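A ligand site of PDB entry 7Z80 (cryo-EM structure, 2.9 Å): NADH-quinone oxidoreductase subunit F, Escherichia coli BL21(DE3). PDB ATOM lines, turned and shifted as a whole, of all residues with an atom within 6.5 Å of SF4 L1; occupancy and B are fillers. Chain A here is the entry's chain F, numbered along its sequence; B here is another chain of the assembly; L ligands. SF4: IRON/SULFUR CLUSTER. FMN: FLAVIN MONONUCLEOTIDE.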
ATOM      1  N   ILE A 179      12.355 -20.016 -11.645  1.00  0.00           N
ATOM      2  CA  ILE A 179      11.281 -20.606 -10.835  1.00  0.00           C
ATOM      3  C   ILE A 179      10.547 -19.578  -9.998  1.00  0.00           C
ATOM      4  O   ILE A 179       9.445 -19.859  -9.519  1.00  0.00           O
ATOM      5  CB  ILE A 179      11.875 -21.732  -9.960  1.00  0.00           C
ATOM      6  CG1 ILE A 179      10.801 -22.742  -9.557  1.00  0.00           C
ATOM      7  CG2 ILE A 179      12.569 -21.160  -8.730  1.00  0.00           C
ATOM      8  CD1 ILE A 179       9.959 -23.236 -10.709  1.00  0.00           C
ATOM      9  N   ALA A 195      13.139 -19.793  -3.385  1.00  0.00           N
ATOM     10  CA  ALA A 195      11.920 -19.815  -4.186  1.00  0.00           C
ATOM     11  C   ALA A 195      11.485 -21.249  -4.529  1.00  0.00           C
ATOM     12  O   ALA A 195      11.334 -21.625  -5.692  1.00  0.00           O
ATOM     13  CB  ALA A 195      12.103 -18.984  -5.447  1.00  0.00           C
ATOM     14  N   ASN A 196      11.300 -22.035  -3.496  1.00  0.00           N
ATOM     15  CA  ASN A 196      10.631 -23.323  -3.658  1.00  0.00           C
ATOM     16  C   ASN A 196       9.117 -23.089  -3.710  1.00  0.00           C
ATOM     17  O   ASN A 196       8.578 -22.379  -2.858  1.00  0.00           O
ATOM     18  CB  ASN A 196      10.973 -24.268  -2.513  1.00  0.00           C
ATOM     19  CG  ASN A 196      12.439 -24.619  -2.466  1.00  0.00           C
ATOM     20  OD1 ASN A 196      13.129 -24.301  -1.504  1.00  0.00           O
ATOM     21  ND2 ASN A 196      12.919 -25.286  -3.508  1.00  0.00           N
ATOM     22  N   PRO A 197       8.421 -23.662  -4.687  1.00  0.00           N
ATOM     23  CA  PRO A 197       6.964 -23.523  -4.727  1.00  0.00           C
ATOM     24  C   PRO A 197       6.307 -24.296  -3.593  1.00  0.00           C
ATOM     25  O   PRO A 197       6.940 -25.047  -2.844  1.00  0.00           O
ATOM     26  CB  PRO A 197       6.577 -24.105  -6.090  1.00  0.00           C
ATOM     27  CG  PRO A 197       7.714 -24.979  -6.459  1.00  0.00           C
ATOM     28  CD  PRO A 197       8.944 -24.372  -5.870  1.00  0.00           C
ATOM     29  N   GLU A 349      17.499 -24.470 -14.414  1.00  0.00           N
ATOM     30  CA  GLU A 349      16.591 -23.555 -13.730  1.00  0.00           C
ATOM     31  C   GLU A 349      15.631 -24.287 -12.813  1.00  0.00           C
ATOM     32  O   GLU A 349      14.624 -23.715 -12.382  1.00  0.00           O
ATOM     33  CB  GLU A 349      15.837 -22.688 -14.726  1.00  0.00           C
ATOM     34  CG  GLU A 349      16.721 -21.712 -15.465  1.00  0.00           C
ATOM     35  CD  GLU A 349      17.396 -20.719 -14.538  1.00  0.00           C
ATOM     36  OE1 GLU A 349      16.732 -20.237 -13.598  1.00  0.00           O
ATOM     37  OE2 GLU A 349      18.580 -20.409 -14.755  1.00  0.00           O
ATOM     38  N   SER A 350      15.911 -25.555 -12.509  1.00  0.00           N
ATOM     39  CA  SER A 350      15.174 -26.278 -11.490  1.00  0.00           C
ATOM     40  C   SER A 350      15.443 -25.667 -10.114  1.00  0.00           C
ATOM     41  O   SER A 350      16.464 -25.019  -9.888  1.00  0.00           O
ATOM     42  CB  SER A 350      15.580 -27.748 -11.493  1.00  0.00           C
ATOM     43  OG  SER A 350      15.015 -28.440 -10.401  1.00  0.00           O
ATOM     44  N   CYS A 351      14.503 -25.866  -9.211  1.00  0.00           N
ATOM     45  CA  CYS A 351      14.682 -25.383  -7.853  1.00  0.00           C
ATOM     46  C   CYS A 351      15.265 -26.442  -6.928  1.00  0.00           C
ATOM     47  O   CYS A 351      15.796 -26.091  -5.867  1.00  0.00           O
ATOM     48  CB  CYS A 351      13.353 -24.881  -7.286  1.00  0.00           C
ATOM     49  SG  CYS A 351      12.368 -26.140  -6.490  1.00  0.00           S
ATOM     50  N   GLY A 352      15.197 -27.715  -7.312  1.00  0.00           N
ATOM     51  CA  GLY A 352      15.803 -28.783  -6.544  1.00  0.00           C
ATOM     52  C   GLY A 352      14.957 -29.333  -5.420  1.00  0.00           C
ATOM     53  O   GLY A 352      15.483 -30.116  -4.611  1.00  0.00           O
ATOM     54  N   TRP A 353      13.691 -28.938  -5.319  1.00  0.00           N
ATOM     55  CA  TRP A 353      12.868 -29.413  -4.212  1.00  0.00           C
ATOM     56  C   TRP A 353      12.489 -30.875  -4.391  1.00  0.00           C
ATOM     57  O   TRP A 353      12.567 -31.657  -3.445  1.00  0.00           O
ATOM     58  CB  TRP A 353      11.602 -28.556  -4.096  1.00  0.00           C
ATOM     59  CG  TRP A 353      10.633 -29.067  -3.101  1.00  0.00           C
ATOM     60  CD1 TRP A 353       9.449 -29.690  -3.357  1.00  0.00           C
ATOM     61  CD2 TRP A 353      10.753 -29.017  -1.670  1.00  0.00           C
ATOM     62  NE1 TRP A 353       8.822 -30.027  -2.188  1.00  0.00           N
ATOM     63  CE2 TRP A 353       9.607 -29.620  -1.138  1.00  0.00           C
ATOM     64  CE3 TRP A 353      11.725 -28.521  -0.802  1.00  0.00           C
ATOM     65  CZ2 TRP A 353       9.399 -29.740   0.234  1.00  0.00           C
ATOM     66  CZ3 TRP A 353      11.525 -28.632   0.551  1.00  0.00           C
ATOM     67  CH2 TRP A 353      10.366 -29.242   1.058  1.00  0.00           C
ATOM     68  N   CYS A 354      12.072 -31.255  -5.593  1.00  0.00           N
ATOM     69  CA  CYS A 354      11.470 -32.564  -5.772  1.00  0.00           C
ATOM     70  C   CYS A 354      12.258 -33.410  -6.765  1.00  0.00           C
ATOM     71  O   CYS A 354      12.859 -32.891  -7.715  1.00  0.00           O
ATOM     72  CB  CYS A 354       9.992 -32.454  -6.171  1.00  0.00           C
ATOM     73  SG  CYS A 354       9.608 -32.166  -7.886  1.00  0.00           S
ATOM     74  N   THR A 355      12.249 -34.720  -6.508  1.00  0.00           N
ATOM     75  CA  THR A 355      13.170 -35.660  -7.150  1.00  0.00           C
ATOM     76  C   THR A 355      13.077 -35.752  -8.675  1.00  0.00           C
ATOM     77  O   THR A 355      14.127 -35.704  -9.326  1.00  0.00           O
ATOM     78  CB  THR A 355      13.008 -37.037  -6.506  1.00  0.00           C
ATOM     79  OG1 THR A 355      13.367 -36.957  -5.123  1.00  0.00           O
ATOM     80  CG2 THR A 355      13.889 -38.076  -7.189  1.00  0.00           C
ATOM     81  N   PRO A 356      11.889 -35.916  -9.306  1.00  0.00           N
ATOM     82  CA  PRO A 356      11.892 -36.237 -10.749  1.00  0.00           C
ATOM     83  C   PRO A 356      12.503 -35.170 -11.635  1.00  0.00           C
ATOM     84  O   PRO A 356      13.360 -35.484 -12.462  1.00  0.00           O
ATOM     85  CB  PRO A 356      10.404 -36.453 -11.053  1.00  0.00           C
ATOM     86  CG  PRO A 356       9.801 -36.774  -9.774  1.00  0.00           C
ATOM     87  CD  PRO A 356      10.503 -35.878  -8.822  1.00  0.00           C
ATOM     88  N   CYS A 357      12.126 -33.902 -11.438  1.00  0.00           N
ATOM     89  CA  CYS A 357      12.732 -32.813 -12.196  1.00  0.00           C
ATOM     90  C   CYS A 357      14.221 -32.713 -11.910  1.00  0.00           C
ATOM     91  O   CYS A 357      15.040 -32.805 -12.840  1.00  0.00           O
ATOM     92  CB  CYS A 357      11.989 -31.518 -11.864  1.00  0.00           C
ATOM     93  SG  CYS A 357      12.755 -29.899 -12.097  1.00  0.00           S
ATOM     94  N   ARG A 358      14.588 -32.647 -10.628  1.00  0.00           N
ATOM     95  CA  ARG A 358      15.969 -32.401 -10.207  1.00  0.00           C
ATOM     96  C   ARG A 358      16.931 -33.480 -10.688  1.00  0.00           C
ATOM     97  O   ARG A 358      18.050 -33.171 -11.119  1.00  0.00           O
ATOM     98  CB  ARG A 358      16.023 -32.293  -8.681  1.00  0.00           C
ATOM     99  CG  ARG A 358      17.413 -32.414  -8.076  1.00  0.00           C
ATOM    100  CD  ARG A 358      17.367 -32.591  -6.575  1.00  0.00           C
ATOM    101  NE  ARG A 358      17.123 -33.979  -6.207  1.00  0.00           N
ATOM    102  CZ  ARG A 358      16.117 -34.376  -5.432  1.00  0.00           C
ATOM    103  NH1 ARG A 358      15.258 -33.511  -4.917  1.00  0.00           N
ATOM    104  NH2 ARG A 358      15.988 -35.674  -5.171  1.00  0.00           N
ATOM    105  N   LEU A 361      15.820 -34.363 -15.251  1.00  0.00           N
ATOM    106  CA  LEU A 361      16.134 -33.414 -16.295  1.00  0.00           C
ATOM    107  C   LEU A 361      17.624 -33.432 -16.672  1.00  0.00           C
ATOM    108  O   LEU A 361      17.917 -33.382 -17.872  1.00  0.00           O
ATOM    109  CB  LEU A 361      15.677 -32.006 -15.898  1.00  0.00           C
ATOM    110  CG  LEU A 361      14.167 -31.765 -15.923  1.00  0.00           C
ATOM    111  CD1 LEU A 361      13.867 -30.289 -15.787  1.00  0.00           C
ATOM    112  CD2 LEU A 361      13.541 -32.308 -17.199  1.00  0.00           C
ATOM    113  N   LEU A 391       7.425 -37.501 -15.931  1.00  0.00           N
ATOM    114  CA  LEU A 391       7.577 -36.110 -15.488  1.00  0.00           C
ATOM    115  C   LEU A 391       6.367 -35.270 -15.855  1.00  0.00           C
ATOM    116  O   LEU A 391       6.463 -34.040 -15.922  1.00  0.00           O
ATOM    117  CB  LEU A 391       8.848 -35.500 -16.083  1.00  0.00           C
ATOM    118  CG  LEU A 391      10.152 -35.792 -15.336  1.00  0.00           C
ATOM    119  CD1 LEU A 391      11.326 -35.825 -16.284  1.00  0.00           C
ATOM    120  CD2 LEU A 391      10.358 -34.737 -14.315  1.00  0.00           C
ATOM    121  N   THR A 396       5.382 -34.430 -10.443  1.00  0.00           N
ATOM    122  CA  THR A 396       6.305 -33.528  -9.781  1.00  0.00           C
ATOM    123  C   THR A 396       5.554 -32.550  -8.890  1.00  0.00           C
ATOM    124  O   THR A 396       4.325 -32.411  -8.959  1.00  0.00           O
ATOM    125  CB  THR A 396       7.152 -32.775 -10.815  1.00  0.00           C
ATOM    126  OG1 THR A 396       6.317 -31.886 -11.562  1.00  0.00           O
ATOM    127  CG2 THR A 396       7.818 -33.755 -11.746  1.00  0.00           C
ATOM    128  N   PHE A 397       6.314 -31.860  -8.035  1.00  0.00           N
ATOM    129  CA  PHE A 397       5.730 -30.964  -7.054  1.00  0.00           C
ATOM    130  C   PHE A 397       5.086 -29.750  -7.704  1.00  0.00           C
ATOM    131  O   PHE A 397       4.010 -29.303  -7.279  1.00  0.00           O
ATOM    132  CB  PHE A 397       6.794 -30.533  -6.046  1.00  0.00           C
ATOM    133  CG  PHE A 397       6.242 -29.859  -4.834  1.00  0.00           C
ATOM    134  CD1 PHE A 397       5.665 -30.601  -3.815  1.00  0.00           C
ATOM    135  CD2 PHE A 397       6.299 -28.486  -4.692  1.00  0.00           C
ATOM    136  CE1 PHE A 397       5.160 -29.984  -2.697  1.00  0.00           C
ATOM    137  CE2 PHE A 397       5.794 -27.870  -3.574  1.00  0.00           C
ATOM    138  CZ  PHE A 397       5.226 -28.617  -2.570  1.00  0.00           C
ATOM    139  N   CYS A 398       5.708 -29.207  -8.745  1.00  0.00           N
ATOM    140  CA  CYS A 398       5.143 -28.071  -9.457  1.00  0.00           C
ATOM    141  C   CYS A 398       5.103 -28.347 -10.951  1.00  0.00           C
ATOM    142  O   CYS A 398       5.392 -29.466 -11.380  1.00  0.00           O
ATOM    143  CB  CYS A 398       5.929 -26.788  -9.145  1.00  0.00           C
ATOM    144  SG  CYS A 398       7.309 -26.452 -10.247  1.00  0.00           S
ATOM    145  N   ALA A 399       4.752 -27.339 -11.750  1.00  0.00           N
ATOM    146  CA  ALA A 399       4.523 -27.525 -13.179  1.00  0.00           C
ATOM    147  C   ALA A 399       5.713 -27.105 -14.035  1.00  0.00           C
ATOM    148  O   ALA A 399       5.561 -26.919 -15.240  1.00  0.00           O
ATOM    149  CB  ALA A 399       3.261 -26.768 -13.612  1.00  0.00           C
ATOM    150  N   HIS A 400       6.890 -26.931 -13.420  1.00  0.00           N
ATOM    151  CA  HIS A 400       8.083 -26.614 -14.196  1.00  0.00           C
ATOM    152  C   HIS A 400       8.501 -27.786 -15.078  1.00  0.00           C
ATOM    153  O   HIS A 400       8.868 -27.594 -16.239  1.00  0.00           O
ATOM    154  CB  HIS A 400       9.220 -26.221 -13.238  1.00  0.00           C
ATOM    155  CG  HIS A 400      10.582 -26.239 -13.858  1.00  0.00           C
ATOM    156  ND1 HIS A 400      11.120 -25.145 -14.505  1.00  0.00           N
ATOM    157  CD2 HIS A 400      11.527 -27.199 -13.904  1.00  0.00           C
ATOM    158  CE1 HIS A 400      12.324 -25.443 -14.937  1.00  0.00           C
ATOM    159  NE2 HIS A 400      12.602 -26.681 -14.582  1.00  0.00           N
ATOM    160  N   ALA A 401       8.427 -28.999 -14.544  1.00  0.00           N
ATOM    161  CA  ALA A 401       8.874 -30.198 -15.237  1.00  0.00           C
ATOM    162  C   ALA A 401       7.926 -30.728 -16.321  1.00  0.00           C
ATOM    163  O   ALA A 401       8.430 -31.214 -17.342  1.00  0.00           O
ATOM    164  CB  ALA A 401       9.163 -31.301 -14.210  1.00  0.00           C
ATOM    165  N   PRO A 402       6.584 -30.693 -16.174  1.00  0.00           N
ATOM    166  CA  PRO A 402       5.749 -31.025 -17.351  1.00  0.00           C
ATOM    167  C   PRO A 402       5.957 -30.091 -18.533  1.00  0.00           C
ATOM    168  O   PRO A 402       6.035 -30.549 -19.679  1.00  0.00           O
ATOM    169  CB  PRO A 402       4.324 -30.928 -16.797  1.00  0.00           C
ATOM    170  CG  PRO A 402       4.463 -31.234 -15.372  1.00  0.00           C
ATOM    171  CD  PRO A 402       5.755 -30.615 -14.965  1.00  0.00           C
ATOM    172  N   HIS B 176      19.590 -26.173  -8.615  1.00  0.00           N
ATOM    173  CA  HIS B 176      18.851 -27.182  -9.374  1.00  0.00           C
ATOM    174  C   HIS B 176      19.100 -28.630  -8.985  1.00  0.00           C
ATOM    175  O   HIS B 176      18.172 -29.343  -8.612  1.00  0.00           O
ATOM    176  CB  HIS B 176      19.215 -26.996 -10.837  1.00  0.00           C
ATOM    177  CG  HIS B 176      20.612 -26.499 -11.046  1.00  0.00           C
ATOM    178  ND1 HIS B 176      21.699 -27.330 -11.065  1.00  0.00           N
ATOM    179  CD2 HIS B 176      21.102 -25.250 -11.212  1.00  0.00           C
ATOM    180  CE1 HIS B 176      22.801 -26.622 -11.237  1.00  0.00           C
ATOM    181  NE2 HIS B 176      22.462 -25.354 -11.341  1.00  0.00           N
HETATM  182 FE1  SF4 L   1      10.105 -29.982  -8.484  1.00  0.00          FE
HETATM  183 FE2  SF4 L   1      11.531 -28.882 -10.402  1.00  0.00          FE
HETATM  184 FE3  SF4 L   1       9.202 -27.661  -9.609  1.00  0.00          FE
HETATM  185 FE4  SF4 L   1      11.338 -27.539  -8.042  1.00  0.00          FE
HETATM  186  S1  SF4 L   1      11.191 -26.619 -10.145  1.00  0.00           S
HETATM  187  S2  SF4 L   1       9.227 -28.170  -7.370  1.00  0.00           S
HETATM  188  S3  SF4 L   1      12.370 -29.570  -8.371  1.00  0.00           S
HETATM  189  S4  SF4 L   1       9.390 -29.695 -10.645  1.00  0.00           S
HETATM  190  N1  FMN L   2       3.404 -16.423 -14.516  1.00  0.00           N
HETATM  191  C2  FMN L   2       3.820 -15.143 -14.809  1.00  0.00           C
HETATM  192  O2  FMN L   2       2.986 -14.242 -14.907  1.00  0.00           O
HETATM  193  N3  FMN L   2       5.159 -14.867 -14.976  1.00  0.00           N
HETATM  194  C4  FMN L   2       6.078 -15.890 -14.860  1.00  0.00           C
HETATM  195  O4  FMN L   2       7.274 -15.660 -15.019  1.00  0.00           O
HETATM  196  C4A FMN L   2       5.661 -17.171 -14.568  1.00  0.00           C
HETATM  197  N5  FMN L   2       6.580 -18.189 -14.461  1.00  0.00           N
HETATM  198  C5A FMN L   2       6.164 -19.461 -14.163  1.00  0.00           C
HETATM  199  C6  FMN L   2       7.115 -20.463 -14.050  1.00  0.00           C
HETATM  200  C7  FMN L   2       6.717 -21.754 -13.764  1.00  0.00           C
HETATM  201  C7M FMN L   2       7.754 -22.824 -13.650  1.00  0.00           C
HETATM  202  C8  FMN L   2       5.369 -22.047 -13.583  1.00  0.00           C
HETATM  203  C8M FMN L   2       4.936 -23.448 -13.276  1.00  0.00           C
HETATM  204  C9  FMN L   2       4.418 -21.045 -13.696  1.00  0.00           C
HETATM  205  C9A FMN L   2       4.817 -19.740 -13.986  1.00  0.00           C
HETATM  206  N10 FMN L   2       3.887 -18.717 -14.101  1.00  0.00           N
HETATM  207  C10 FMN L   2       4.314 -17.437 -14.394  1.00  0.00           C
HETATM  208  C1' FMN L   2       2.412 -18.962 -13.917  1.00  0.00           C
HETATM  209  C2' FMN L   2       2.012 -18.715 -12.462  1.00  0.00           C
HETATM  210  O2' FMN L   2       1.955 -19.935 -11.773  1.00  0.00           O
HETATM  211  C3' FMN L   2       0.666 -18.010 -12.344  1.00  0.00           C
HETATM  212  O3' FMN L   2      -0.160 -18.405 -13.408  1.00  0.00           O
HETATM  213  C4' FMN L   2       0.825 -16.495 -12.360  1.00  0.00           C
HETATM  214  O4' FMN L   2       1.541 -16.092 -11.203  1.00  0.00           O
HETATM  215  C5' FMN L   2      -0.517 -15.784 -12.399  1.00  0.00           C
HETATM  216  O5' FMN L   2      -1.251 -16.283 -13.482  1.00  0.00           O
HETATM  217  P   FMN L   2      -2.583 -15.532 -13.993  1.00  0.00           P
HETATM  218  O1P FMN L   2      -2.227 -14.658 -15.162  1.00  0.00           O
HETATM  219  O2P FMN L   2      -3.588 -16.582 -14.410  1.00  0.00           O
HETATM  220  O3P FMN L   2      -3.156 -14.682 -12.889  1.00  0.00           O
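The backbone NH (N) of Cys 354 sits close to a sulfur (S3) of SF4 L1 (3.3 Å).
FE1 of SF4 L1 is bound by SG of Cys 354, at 2.3 Å.
SG of Cys 357 binds FE2 of SF4 L1 (2.3 Å).
The backbone NH (N) of Cys 351 sits close to a sulfur (S1) of SF4 L1 (3.5 Å).
The side-chain sulfur (SG) of Cys 351 binds an iron atom (FE4) of SF4 L1 (2.3 Å).
The side-chain sulfur (SG) of Cys 398 is bound to an iron atom (FE3) of SF4 L1 (2.3 Å).
S3 of SF4 L1 lies close to N of Trp 353 (3.4 Å).
The side-chain hydroxyl of Ser 350 lies close to a sulfur (S3) of SF4 L1, 3.5 Å away.
A sulfur (S3) of SF4 L1 lies close to the backbone NH (N) of Gly 352, at 3.5 Å.
The backbone NH of Phe 397 lies close to the side-chain sulfur of Cys 354 (3.3 Å).
The side-chain sulfur (SG) of Cys 357 sits close to the side-chain hydroxyl (OG) of Ser 350 (3.2 Å).
The side-chain sulfur (SG) of Cys 351 sits close to the backbone NH (N) of Trp 353, 3.3 Å away.
SG of Cys 351 sits close to ND2 of Asn 196 (3.2 Å).
The side-chain sulfur (SG) of Cys 398 sits close to the backbone NH (N) of His 400 (3.2 Å).
The backbone carbonyl oxygen of Cys 398 is in hydrogen-bond range of the side-chain hydroxyl of Thr 396 (2.6 Å).
The side-chain hydroxyl of Ser 350 lies within hydrogen-bond range of the backbone NH of Gly 352 (3.2 Å).
The guanidinium group of Arg 358 is in hydrogen-bond range of the backbone carbonyl oxygen of Gly 352, at 3.4 Å.
Residues that only touch SF4 L1: Ile 179, Pro 197, Thr 396, Phe 397, His 400 and Ala 401.
Hydrophobic or aromatic side chains within 4 Å of SF4 L1: Ile 179, Pro 197, Phe 397, His 400 and Ala 401.
Along chain A the residues within 4 Å of SF4 L1 span positions 179 to 401.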
